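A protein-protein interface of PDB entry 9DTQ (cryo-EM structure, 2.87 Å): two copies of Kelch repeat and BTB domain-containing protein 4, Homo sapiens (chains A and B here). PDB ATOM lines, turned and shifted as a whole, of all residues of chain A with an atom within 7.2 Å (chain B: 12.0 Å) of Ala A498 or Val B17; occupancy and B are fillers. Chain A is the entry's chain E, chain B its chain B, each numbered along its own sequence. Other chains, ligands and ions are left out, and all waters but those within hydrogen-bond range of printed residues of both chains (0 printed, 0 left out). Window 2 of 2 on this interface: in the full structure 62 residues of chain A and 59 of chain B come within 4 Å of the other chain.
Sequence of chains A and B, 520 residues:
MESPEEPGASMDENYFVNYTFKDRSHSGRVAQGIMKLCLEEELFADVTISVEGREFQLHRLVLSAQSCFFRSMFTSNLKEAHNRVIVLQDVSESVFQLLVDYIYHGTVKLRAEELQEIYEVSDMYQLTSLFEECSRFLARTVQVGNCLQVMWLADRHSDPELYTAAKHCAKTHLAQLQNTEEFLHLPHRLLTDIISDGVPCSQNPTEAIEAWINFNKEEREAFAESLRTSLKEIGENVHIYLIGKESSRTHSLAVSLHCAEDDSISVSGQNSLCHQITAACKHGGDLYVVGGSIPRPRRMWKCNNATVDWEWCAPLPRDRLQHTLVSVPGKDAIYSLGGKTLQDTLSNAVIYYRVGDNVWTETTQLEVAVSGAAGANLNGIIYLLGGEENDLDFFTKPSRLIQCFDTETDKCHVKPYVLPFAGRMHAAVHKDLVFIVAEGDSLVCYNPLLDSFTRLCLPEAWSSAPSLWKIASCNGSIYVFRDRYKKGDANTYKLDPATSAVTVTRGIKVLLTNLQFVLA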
ATOM      1  N   LYS A 109     -15.039  14.720 -28.964  1.00  0.00           N
ATOM      2  CA  LYS A 109     -15.889  13.547 -29.144  1.00  0.00           C
ATOM      3  C   LYS A 109     -16.069  12.871 -27.790  1.00  0.00           C
ATOM      4  O   LYS A 109     -15.131  12.262 -27.264  1.00  0.00           O
ATOM      5  CB  LYS A 109     -15.283  12.588 -30.165  1.00  0.00           C
ATOM      6  CG  LYS A 109     -16.164  11.400 -30.500  1.00  0.00           C
ATOM      7  CD  LYS A 109     -16.420  11.309 -31.995  1.00  0.00           C
ATOM      8  CE  LYS A 109     -17.740  10.617 -32.287  1.00  0.00           C
ATOM      9  NZ  LYS A 109     -18.007   9.507 -31.334  1.00  0.00           N
ATOM     10  N   LEU A 110     -17.274  12.968 -27.236  1.00  0.00           N
ATOM     11  CA  LEU A 110     -17.554  12.486 -25.892  1.00  0.00           C
ATOM     12  C   LEU A 110     -18.020  11.038 -25.919  1.00  0.00           C
ATOM     13  O   LEU A 110     -18.846  10.654 -26.749  1.00  0.00           O
ATOM     14  CB  LEU A 110     -18.615  13.360 -25.222  1.00  0.00           C
ATOM     15  CG  LEU A 110     -18.242  14.825 -25.002  1.00  0.00           C
ATOM     16  CD1 LEU A 110     -19.440  15.611 -24.512  1.00  0.00           C
ATOM     17  CD2 LEU A 110     -17.091  14.939 -24.023  1.00  0.00           C
ATOM     18  N   ARG A 111     -17.485  10.238 -25.000  1.00  0.00           N
ATOM     19  CA  ARG A 111     -17.823   8.829 -24.884  1.00  0.00           C
ATOM     20  C   ARG A 111     -18.158   8.503 -23.438  1.00  0.00           C
ATOM     21  O   ARG A 111     -17.640   9.128 -22.509  1.00  0.00           O
ATOM     22  CB  ARG A 111     -16.678   7.934 -25.363  1.00  0.00           C
ATOM     23  CG  ARG A 111     -16.644   7.718 -26.864  1.00  0.00           C
ATOM     24  CD  ARG A 111     -15.238   7.886 -27.413  1.00  0.00           C
ATOM     25  NE  ARG A 111     -14.234   7.347 -26.505  1.00  0.00           N
ATOM     26  CZ  ARG A 111     -13.944   6.059 -26.387  1.00  0.00           C
ATOM     27  NH1 ARG A 111     -14.568   5.141 -27.108  1.00  0.00           N
ATOM     28  NH2 ARG A 111     -13.007   5.681 -25.524  1.00  0.00           N
ATOM     29  N   ALA A 112     -19.031   7.512 -23.254  1.00  0.00           N
ATOM     30  CA  ALA A 112     -19.487   7.147 -21.920  1.00  0.00           C
ATOM     31  C   ALA A 112     -18.440   6.381 -21.122  1.00  0.00           C
ATOM     32  O   ALA A 112     -18.558   6.298 -19.896  1.00  0.00           O
ATOM     33  CB  ALA A 112     -20.769   6.320 -22.012  1.00  0.00           C
ATOM     34  N   GLU A 113     -17.427   5.821 -21.783  1.00  0.00           N
ATOM     35  CA  GLU A 113     -16.392   5.081 -21.069  1.00  0.00           C
ATOM     36  C   GLU A 113     -15.405   6.002 -20.363  1.00  0.00           C
ATOM     37  O   GLU A 113     -14.856   5.628 -19.321  1.00  0.00           O
ATOM     38  CB  GLU A 113     -15.652   4.152 -22.032  1.00  0.00           C
ATOM     39  CG  GLU A 113     -16.573   3.271 -22.858  1.00  0.00           C
ATOM     40  CD  GLU A 113     -16.552   3.622 -24.330  1.00  0.00           C
ATOM     41  OE1 GLU A 113     -15.462   3.944 -24.847  1.00  0.00           O
ATOM     42  OE2 GLU A 113     -17.624   3.580 -24.970  1.00  0.00           O
ATOM     43  N   LEU A 115     -16.306   9.226 -19.472  1.00  0.00           N
ATOM     44  CA  LEU A 115     -17.117  10.384 -19.111  1.00  0.00           C
ATOM     45  C   LEU A 115     -16.741  10.945 -17.745  1.00  0.00           C
ATOM     46  O   LEU A 115     -16.612  12.164 -17.586  1.00  0.00           O
ATOM     47  CB  LEU A 115     -18.595  10.006 -19.146  1.00  0.00           C
ATOM     48  CG  LEU A 115     -19.597  11.148 -19.284  1.00  0.00           C
ATOM     49  CD1 LEU A 115     -19.130  12.140 -20.331  1.00  0.00           C
ATOM     50  CD2 LEU A 115     -20.957  10.586 -19.632  1.00  0.00           C
ATOM     51  N   PHE A 137     -24.359  15.099 -20.088  1.00  0.00           N
ATOM     52  CA  PHE A 137     -24.204  13.722 -20.548  1.00  0.00           C
ATOM     53  C   PHE A 137     -24.294  12.743 -19.381  1.00  0.00           C
ATOM     54  O   PHE A 137     -24.952  11.703 -19.480  1.00  0.00           O
ATOM     55  CB  PHE A 137     -22.867  13.584 -21.284  1.00  0.00           C
ATOM     56  CG  PHE A 137     -22.716  12.312 -22.090  1.00  0.00           C
ATOM     57  CD1 PHE A 137     -23.724  11.368 -22.156  1.00  0.00           C
ATOM     58  CD2 PHE A 137     -21.550  12.076 -22.794  1.00  0.00           C
ATOM     59  CE1 PHE A 137     -23.564  10.217 -22.893  1.00  0.00           C
ATOM     60  CE2 PHE A 137     -21.391  10.927 -23.534  1.00  0.00           C
ATOM     61  CZ  PHE A 137     -22.397   9.999 -23.582  1.00  0.00           C
ATOM     62  N   ARG A 140     -27.782  12.401 -18.263  1.00  0.00           N
ATOM     63  CA  ARG A 140     -28.591  11.707 -19.260  1.00  0.00           C
ATOM     64  C   ARG A 140     -28.561  10.198 -19.053  1.00  0.00           C
ATOM     65  O   ARG A 140     -29.592   9.527 -19.172  1.00  0.00           O
ATOM     66  CB  ARG A 140     -28.096  12.060 -20.662  1.00  0.00           C
ATOM     67  CG  ARG A 140     -29.176  12.149 -21.711  1.00  0.00           C
ATOM     68  CD  ARG A 140     -28.602  12.025 -23.110  1.00  0.00           C
ATOM     69  NE  ARG A 140     -27.380  12.798 -23.299  1.00  0.00           N
ATOM     70  CZ  ARG A 140     -27.341  14.113 -23.468  1.00  0.00           C
ATOM     71  NH1 ARG A 140     -28.441  14.846 -23.443  1.00  0.00           N
ATOM     72  NH2 ARG A 140     -26.170  14.707 -23.670  1.00  0.00           N
ATOM     73  N   THR A 141     -27.390   9.645 -18.739  1.00  0.00           N
ATOM     74  CA  THR A 141     -27.177   8.204 -18.733  1.00  0.00           C
ATOM     75  C   THR A 141     -27.064   7.622 -17.326  1.00  0.00           C
ATOM     76  O   THR A 141     -26.396   6.600 -17.140  1.00  0.00           O
ATOM     77  CB  THR A 141     -25.927   7.858 -19.541  1.00  0.00           C
ATOM     78  OG1 THR A 141     -24.776   8.437 -18.917  1.00  0.00           O
ATOM     79  CG2 THR A 141     -26.045   8.403 -20.949  1.00  0.00           C
ATOM     80  N   GLN A 143     -28.267   5.579 -14.042  1.00  0.00           N
ATOM     81  CA  GLN A 143     -29.087   4.388 -13.858  1.00  0.00           C
ATOM     82  C   GLN A 143     -28.854   3.849 -12.450  1.00  0.00           C
ATOM     83  O   GLN A 143     -28.203   4.493 -11.622  1.00  0.00           O
ATOM     84  CB  GLN A 143     -28.775   3.346 -14.939  1.00  0.00           C
ATOM     85  CG  GLN A 143     -27.449   2.630 -14.748  1.00  0.00           C
ATOM     86  CD  GLN A 143     -27.002   1.889 -15.989  1.00  0.00           C
ATOM     87  OE1 GLN A 143     -27.733   1.808 -16.974  1.00  0.00           O
ATOM     88  NE2 GLN A 143     -25.796   1.338 -15.945  1.00  0.00           N
ATOM     89  N   HIS A 430     -37.722  12.895 -23.557  1.00  0.00           N
ATOM     90  CA  HIS A 430     -37.056  11.879 -22.746  1.00  0.00           C
ATOM     91  C   HIS A 430     -35.654  12.369 -22.421  1.00  0.00           C
ATOM     92  O   HIS A 430     -34.780  12.354 -23.292  1.00  0.00           O
ATOM     93  CB  HIS A 430     -37.005  10.540 -23.480  1.00  0.00           C
ATOM     94  CG  HIS A 430     -36.354   9.442 -22.699  1.00  0.00           C
ATOM     95  ND1 HIS A 430     -35.284   8.721 -23.181  1.00  0.00           N
ATOM     96  CD2 HIS A 430     -36.629   8.932 -21.475  1.00  0.00           C
ATOM     97  CE1 HIS A 430     -34.921   7.822 -22.285  1.00  0.00           C
ATOM     98  NE2 HIS A 430     -35.722   7.927 -21.241  1.00  0.00           N
ATOM     99  N   GLY A 476     -36.517   5.816 -18.440  1.00  0.00           N
ATOM    100  CA  GLY A 476     -35.356   5.277 -19.119  1.00  0.00           C
ATOM    101  C   GLY A 476     -35.652   4.314 -20.241  1.00  0.00           C
ATOM    102  O   GLY A 476     -34.724   3.697 -20.771  1.00  0.00           O
ATOM    103  N   LEU A 495     -38.225   0.249 -26.380  1.00  0.00           N
ATOM    104  CA  LEU A 495     -36.928   0.602 -26.938  1.00  0.00           C
ATOM    105  C   LEU A 495     -36.033   1.163 -25.845  1.00  0.00           C
ATOM    106  O   LEU A 495     -36.458   2.023 -25.068  1.00  0.00           O
ATOM    107  CB  LEU A 495     -37.080   1.620 -28.069  1.00  0.00           C
ATOM    108  CG  LEU A 495     -35.841   2.470 -28.341  1.00  0.00           C
ATOM    109  CD1 LEU A 495     -34.860   1.702 -29.202  1.00  0.00           C
ATOM    110  CD2 LEU A 495     -36.224   3.781 -28.997  1.00  0.00           C
ATOM    111  N   ASP A 496     -34.799   0.672 -25.786  1.00  0.00           N
ATOM    112  CA  ASP A 496     -33.797   1.228 -24.888  1.00  0.00           C
ATOM    113  C   ASP A 496     -32.832   2.067 -25.710  1.00  0.00           C
ATOM    114  O   ASP A 496     -32.049   1.508 -26.495  1.00  0.00           O
ATOM    115  CB  ASP A 496     -33.052   0.120 -24.144  1.00  0.00           C
ATOM    116  CG  ASP A 496     -31.777   0.611 -23.496  1.00  0.00           C
ATOM    117  OD1 ASP A 496     -31.861   1.321 -22.472  1.00  0.00           O
ATOM    118  OD2 ASP A 496     -30.688   0.287 -24.009  1.00  0.00           O
ATOM    119  N   PRO A 497     -32.852   3.397 -25.581  1.00  0.00           N
ATOM    120  CA  PRO A 497     -32.062   4.238 -26.494  1.00  0.00           C
ATOM    121  C   PRO A 497     -30.560   4.051 -26.376  1.00  0.00           C
ATOM    122  O   PRO A 497     -29.840   4.400 -27.319  1.00  0.00           O
ATOM    123  CB  PRO A 497     -32.479   5.663 -26.108  1.00  0.00           C
ATOM    124  CG  PRO A 497     -32.979   5.549 -24.712  1.00  0.00           C
ATOM    125  CD  PRO A 497     -33.594   4.194 -24.590  1.00  0.00           C
ATOM    126  N   ALA A 498     -30.062   3.519 -25.259  1.00  0.00           N
ATOM    127  CA  ALA A 498     -28.620   3.373 -25.093  1.00  0.00           C
ATOM    128  C   ALA A 498     -28.045   2.361 -26.077  1.00  0.00           C
ATOM    129  O   ALA A 498     -27.077   2.654 -26.787  1.00  0.00           O
ATOM    130  CB  ALA A 498     -28.297   2.971 -23.654  1.00  0.00           C
ATOM    131  N   THR A 499     -28.635   1.169 -26.149  1.00  0.00           N
ATOM    132  CA  THR A 499     -28.143   0.117 -27.031  1.00  0.00           C
ATOM    133  C   THR A 499     -29.036  -0.099 -28.247  1.00  0.00           C
ATOM    134  O   THR A 499     -28.751  -0.984 -29.060  1.00  0.00           O
ATOM    135  CB  THR A 499     -27.978  -1.193 -26.258  1.00  0.00           C
ATOM    136  OG1 THR A 499     -27.202  -2.113 -27.036  1.00  0.00           O
ATOM    137  CG2 THR A 499     -29.329  -1.812 -25.959  1.00  0.00           C
ATOM    138  N   SER A 500     -30.102   0.691 -28.390  1.00  0.00           N
ATOM    139  CA  SER A 500     -30.984   0.644 -29.560  1.00  0.00           C
ATOM    140  C   SER A 500     -31.593  -0.744 -29.756  1.00  0.00           C
ATOM    141  O   SER A 500     -31.768  -1.210 -30.883  1.00  0.00           O
ATOM    142  CB  SER A 500     -30.246   1.095 -30.823  1.00  0.00           C
ATOM    143  OG  SER A 500     -30.333   2.499 -30.991  1.00  0.00           O
ATOM    144  N   ALA A 501     -31.923  -1.406 -28.653  1.00  0.00           N
ATOM    145  CA  ALA A 501     -32.538  -2.726 -28.686  1.00  0.00           C
ATOM    146  C   ALA A 501     -34.044  -2.577 -28.521  1.00  0.00           C
ATOM    147  O   ALA A 501     -34.512  -2.034 -27.515  1.00  0.00           O
ATOM    148  CB  ALA A 501     -31.966  -3.627 -27.593  1.00  0.00           C
ATOM    149  N   SER B  10     -22.524  10.226 -37.989  1.00  0.00           N
ATOM    150  CA  SER B  10     -23.820  10.776 -37.610  1.00  0.00           C
ATOM    151  C   SER B  10     -24.892   9.688 -37.622  1.00  0.00           C
ATOM    152  O   SER B  10     -26.033   9.916 -37.214  1.00  0.00           O
ATOM    153  CB  SER B  10     -24.208  11.921 -38.547  1.00  0.00           C
ATOM    154  OG  SER B  10     -23.290  12.995 -38.444  1.00  0.00           O
ATOM    155  N   MET B  11     -24.515   8.504 -38.102  1.00  0.00           N
ATOM    156  CA  MET B  11     -25.382   7.334 -38.065  1.00  0.00           C
ATOM    157  C   MET B  11     -25.123   6.443 -36.862  1.00  0.00           C
ATOM    158  O   MET B  11     -26.067   5.861 -36.319  1.00  0.00           O
ATOM    159  CB  MET B  11     -25.218   6.508 -39.345  1.00  0.00           C
ATOM    160  CG  MET B  11     -26.348   6.674 -40.348  1.00  0.00           C
ATOM    161  SD  MET B  11     -27.953   6.199 -39.673  1.00  0.00           S
ATOM    162  CE  MET B  11     -28.986   7.525 -40.288  1.00  0.00           C
ATOM    163  N   ASP B  12     -23.868   6.321 -36.436  1.00  0.00           N
ATOM    164  CA  ASP B  12     -23.516   5.622 -35.210  1.00  0.00           C
ATOM    165  C   ASP B  12     -23.450   6.556 -34.012  1.00  0.00           C
ATOM    166  O   ASP B  12     -23.103   6.113 -32.911  1.00  0.00           O
ATOM    167  CB  ASP B  12     -22.173   4.902 -35.379  1.00  0.00           C
ATOM    168  CG  ASP B  12     -22.005   3.743 -34.414  1.00  0.00           C
ATOM    169  OD1 ASP B  12     -23.010   3.333 -33.794  1.00  0.00           O
ATOM    170  OD2 ASP B  12     -20.868   3.245 -34.271  1.00  0.00           O
ATOM    171  N   GLU B  13     -23.774   7.832 -34.200  1.00  0.00           N
ATOM    172  CA  GLU B  13     -23.718   8.822 -33.134  1.00  0.00           C
ATOM    173  C   GLU B  13     -25.051   8.843 -32.398  1.00  0.00           C
ATOM    174  O   GLU B  13     -26.101   9.054 -33.013  1.00  0.00           O
ATOM    175  CB  GLU B  13     -23.404  10.203 -33.706  1.00  0.00           C
ATOM    176  CG  GLU B  13     -22.075  10.777 -33.259  1.00  0.00           C
ATOM    177  CD  GLU B  13     -21.779  12.118 -33.896  1.00  0.00           C
ATOM    178  OE1 GLU B  13     -22.466  13.103 -33.555  1.00  0.00           O
ATOM    179  OE2 GLU B  13     -20.858  12.189 -34.735  1.00  0.00           O
ATOM    180  N   ASN B  14     -25.011   8.617 -31.088  1.00  0.00           N
ATOM    181  CA  ASN B  14     -26.199   8.738 -30.258  1.00  0.00           C
ATOM    182  C   ASN B  14     -25.812   9.337 -28.917  1.00  0.00           C
ATOM    183  O   ASN B  14     -24.758   9.017 -28.363  1.00  0.00           O
ATOM    184  CB  ASN B  14     -26.906   7.386 -30.070  1.00  0.00           C
ATOM    185  CG  ASN B  14     -26.103   6.413 -29.246  1.00  0.00           C
ATOM    186  OD1 ASN B  14     -24.881   6.357 -29.349  1.00  0.00           O
ATOM    187  ND2 ASN B  14     -26.790   5.625 -28.432  1.00  0.00           N
ATOM    188  N   TYR B  15     -26.677  10.207 -28.399  1.00  0.00           N
ATOM    189  CA  TYR B  15     -26.386  11.000 -27.213  1.00  0.00           C
ATOM    190  C   TYR B  15     -26.321  10.180 -25.934  1.00  0.00           C
ATOM    191  O   TYR B  15     -26.119  10.761 -24.865  1.00  0.00           O
ATOM    192  CB  TYR B  15     -27.430  12.106 -27.069  1.00  0.00           C
ATOM    193  CG  TYR B  15     -27.591  12.949 -28.312  1.00  0.00           C
ATOM    194  CD1 TYR B  15     -26.538  13.705 -28.799  1.00  0.00           C
ATOM    195  CD2 TYR B  15     -28.796  12.983 -29.000  1.00  0.00           C
ATOM    196  CE1 TYR B  15     -26.679  14.474 -29.933  1.00  0.00           C
ATOM    197  CE2 TYR B  15     -28.945  13.752 -30.137  1.00  0.00           C
ATOM    198  CZ  TYR B  15     -27.884  14.493 -30.598  1.00  0.00           C
ATOM    199  OH  TYR B  15     -28.023  15.260 -31.728  1.00  0.00           O
ATOM    200  N   PHE B  16     -26.486   8.861 -26.004  1.00  0.00           N
ATOM    201  CA  PHE B  16     -26.432   8.012 -24.825  1.00  0.00           C
ATOM    202  C   PHE B  16     -25.177   7.156 -24.755  1.00  0.00           C
ATOM    203  O   PHE B  16     -24.918   6.558 -23.705  1.00  0.00           O
ATOM    204  CB  PHE B  16     -27.668   7.104 -24.771  1.00  0.00           C
ATOM    205  CG  PHE B  16     -28.939   7.831 -24.443  1.00  0.00           C
ATOM    206  CD1 PHE B  16     -29.656   8.479 -25.433  1.00  0.00           C
ATOM    207  CD2 PHE B  16     -29.415   7.867 -23.147  1.00  0.00           C
ATOM    208  CE1 PHE B  16     -30.822   9.148 -25.135  1.00  0.00           C
ATOM    209  CE2 PHE B  16     -30.579   8.535 -22.843  1.00  0.00           C
ATOM    210  CZ  PHE B  16     -31.284   9.177 -23.839  1.00  0.00           C
ATOM    211  N   VAL B  17     -24.398   7.073 -25.833  1.00  0.00           N
ATOM    212  CA  VAL B  17     -23.157   6.307 -25.835  1.00  0.00           C
ATOM    213  C   VAL B  17     -21.995   7.195 -26.257  1.00  0.00           C
ATOM    214  O   VAL B  17     -21.015   7.336 -25.519  1.00  0.00           O
ATOM    215  CB  VAL B  17     -23.260   5.073 -26.748  1.00  0.00           C
ATOM    216  CG1 VAL B  17     -21.960   4.294 -26.723  1.00  0.00           C
ATOM    217  CG2 VAL B  17     -24.402   4.192 -26.306  1.00  0.00           C
ATOM    218  N   ASN B  18     -22.086   7.796 -27.441  1.00  0.00           N
ATOM    219  CA  ASN B  18     -21.011   8.658 -27.911  1.00  0.00           C
ATOM    220  C   ASN B  18     -21.542   9.640 -28.944  1.00  0.00           C
ATOM    221  O   ASN B  18     -22.390   9.290 -29.766  1.00  0.00           O
ATOM    222  CB  ASN B  18     -19.847   7.846 -28.499  1.00  0.00           C
ATOM    223  CG  ASN B  18     -20.291   6.830 -29.535  1.00  0.00           C
ATOM    224  OD1 ASN B  18     -21.453   6.786 -29.933  1.00  0.00           O
ATOM    225  ND2 ASN B  18     -19.355   6.000 -29.976  1.00  0.00           N
ATOM    226  N   TYR B  19     -21.029  10.866 -28.896  1.00  0.00           N
ATOM    227  CA  TYR B  19     -21.408  11.892 -29.853  1.00  0.00           C
ATOM    228  C   TYR B  19     -20.339  12.973 -29.858  1.00  0.00           C
ATOM    229  O   TYR B  19     -19.502  13.049 -28.956  1.00  0.00           O
ATOM    230  CB  TYR B  19     -22.785  12.485 -29.535  1.00  0.00           C
ATOM    231  CG  TYR B  19     -22.886  13.169 -28.191  1.00  0.00           C
ATOM    232  CD1 TYR B  19     -23.035  12.436 -27.023  1.00  0.00           C
ATOM    233  CD2 TYR B  19     -22.845  14.552 -28.093  1.00  0.00           C
ATOM    234  CE1 TYR B  19     -23.133  13.057 -25.801  1.00  0.00           C
ATOM    235  CE2 TYR B  19     -22.942  15.180 -26.874  1.00  0.00           C
ATOM    236  CZ  TYR B  19     -23.084  14.429 -25.734  1.00  0.00           C
ATOM    237  OH  TYR B  19     -23.181  15.057 -24.516  1.00  0.00           O
ATOM    238  N   THR B  20     -20.378  13.807 -30.892  1.00  0.00           N
ATOM    239  CA  THR B  20     -19.426  14.898 -31.050  1.00  0.00           C
ATOM    240  C   THR B  20     -20.029  16.176 -30.482  1.00  0.00           C
ATOM    241  O   THR B  20     -21.141  16.564 -30.859  1.00  0.00           O
ATOM    242  CB  THR B  20     -19.054  15.080 -32.522  1.00  0.00           C
ATOM    243  OG1 THR B  20     -18.042  14.132 -32.882  1.00  0.00           O
ATOM    244  CG2 THR B  20     -18.531  16.483 -32.777  1.00  0.00           C
ATOM    245  N   PHE B  21     -19.303  16.822 -29.574  1.00  0.00           N
ATOM    246  CA  PHE B  21     -19.728  18.071 -28.960  1.00  0.00           C
ATOM    247  C   PHE B  21     -18.884  19.202 -29.530  1.00  0.00           C
ATOM    248  O   PHE B  21     -17.659  19.202 -29.379  1.00  0.00           O
ATOM    249  CB  PHE B  21     -19.596  18.008 -27.439  1.00  0.00           C
ATOM    250  CG  PHE B  21     -19.625  19.353 -26.766  1.00  0.00           C
ATOM    251  CD1 PHE B  21     -20.746  20.160 -26.846  1.00  0.00           C
ATOM    252  CD2 PHE B  21     -18.536  19.804 -26.040  1.00  0.00           C
ATOM    253  CE1 PHE B  21     -20.775  21.393 -26.227  1.00  0.00           C
ATOM    254  CE2 PHE B  21     -18.562  21.036 -25.419  1.00  0.00           C
ATOM    255  CZ  PHE B  21     -19.682  21.829 -25.513  1.00  0.00           C
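Printed residues of chain A that touch a printed residue of chain B: Lys A109, Leu A110, Arg A111, Ala A112, Phe A137, Arg A140, Thr A141, Pro A497 and Ala A498.
Hydrophobic or aromatic side chains of chain A that line the printed part of chain B: Leu A110, Ala A112, Phe A137 and Pro A497.
Of the 12 printed residues of chain B, 8 touch a printed residue of chain A.
Among the printed residues, 22 pairs touch across the chains.
Of chain B, only Asn B14, Phe B16 and Val B17 come within 4 Å of Ala A498.
Val B17 touches just these residues of chain A: Arg A111, Ala A112, Phe A137 and Ala A498.
Of chain B, only Val B17 (3.0 Å) comes within 4 Å of Ala A112.
Of chain B, only Asn B14 and Phe B16 come within 4 Å of Pro A497.
Of the printed residues of chain A, Phe B16 touches Phe A137 (3.9 Å), Arg A140 (3.9 Å), Thr A141 (3.5 Å), Pro A497 (3.98 Å) and Ala A498 (3.9 Å).
Printed residues of chain B within 4 Å of Leu A110: Asn B18, Tyr B19 and Phe B21.
The nearest residue of chain B that does not touch Ala A498 is Asn B18 (7.2 Å).
The nearest residue of chain A that does not touch Val B17 is Leu A110 (4.2 Å).
Among the printed residues, pairs that only touch across the chains: Lys A109 with Asn B18 (3.8 Å), Lys A109 with Tyr B19 (3.6 Å), Lys A109 with Thr B20 (3.4 Å), Leu A110 with Asn B18 (3.2 Å), Leu A110 with Phe B21 (3.8 Å), Arg A111 with Val B17 (3.6 Å), Arg A111 with Asn B18 (3.6 Å), Phe A137 with Tyr B15 (3.3 Å), Phe A137 with Phe B16 (3.9 Å), Phe A137 with Val B17 (3.6 Å), Phe A137 with Tyr B19 (3.5 Å), Arg A140 with Phe B16 (3.9 Å), Thr A141 with Phe B16 (3.5 Å), Pro A497 with Phe B16 (3.98 Å), Ala A498 with Phe B16 (3.9 Å) and Ala A498 with Val B17 (3.1 Å).
O of Asp B12 lies close to OD1 of Asn B18 (3.5 Å).
The guanidinium group (NH1) of Arg A111 is in salt-bridge range of the side-chain carboxylate (OE1) of Glu A113, at 2.7 Å.
The backbone NH (N) of Thr B20 lies within hydrogen-bond range of the side-chain carboxylate (OE1) of Glu B13, 3.5 Å away.
The side-chain hydroxyl (OG1) of Thr A141 sits at hydrogen-bond distance from the backbone carbonyl oxygen (O) of Phe A137 (3.3 Å).
The backbone carbonyl oxygen of Val B17 lies within hydrogen-bond range of the backbone NH of Ala A112 (3.0 Å).
The side-chain hydroxyl (OH) of Tyr B19 sits at hydrogen-bond distance from the guanidinium group (NH2) of Arg A140.
The guanidinium group (NE) of Arg A140 is in hydrogen-bond range of the backbone carbonyl oxygen (O) of Tyr B15.
ND2 of Asn B14 is in hydrogen-bond range of O of Ala A498 (3.4 Å).
The side-chain amide nitrogen (ND2) of Asn B14 is in hydrogen-bond range of the backbone carbonyl oxygen (O) of Pro A497 (3.5 Å).
O of Tyr B19 is in hydrogen-bond range of N of Leu A110 (2.8 Å).
No position is printed for both chains.
Of the 22 pairs that touch across the chains among the printed residues, none has its exchanged pair printed and touching as well.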
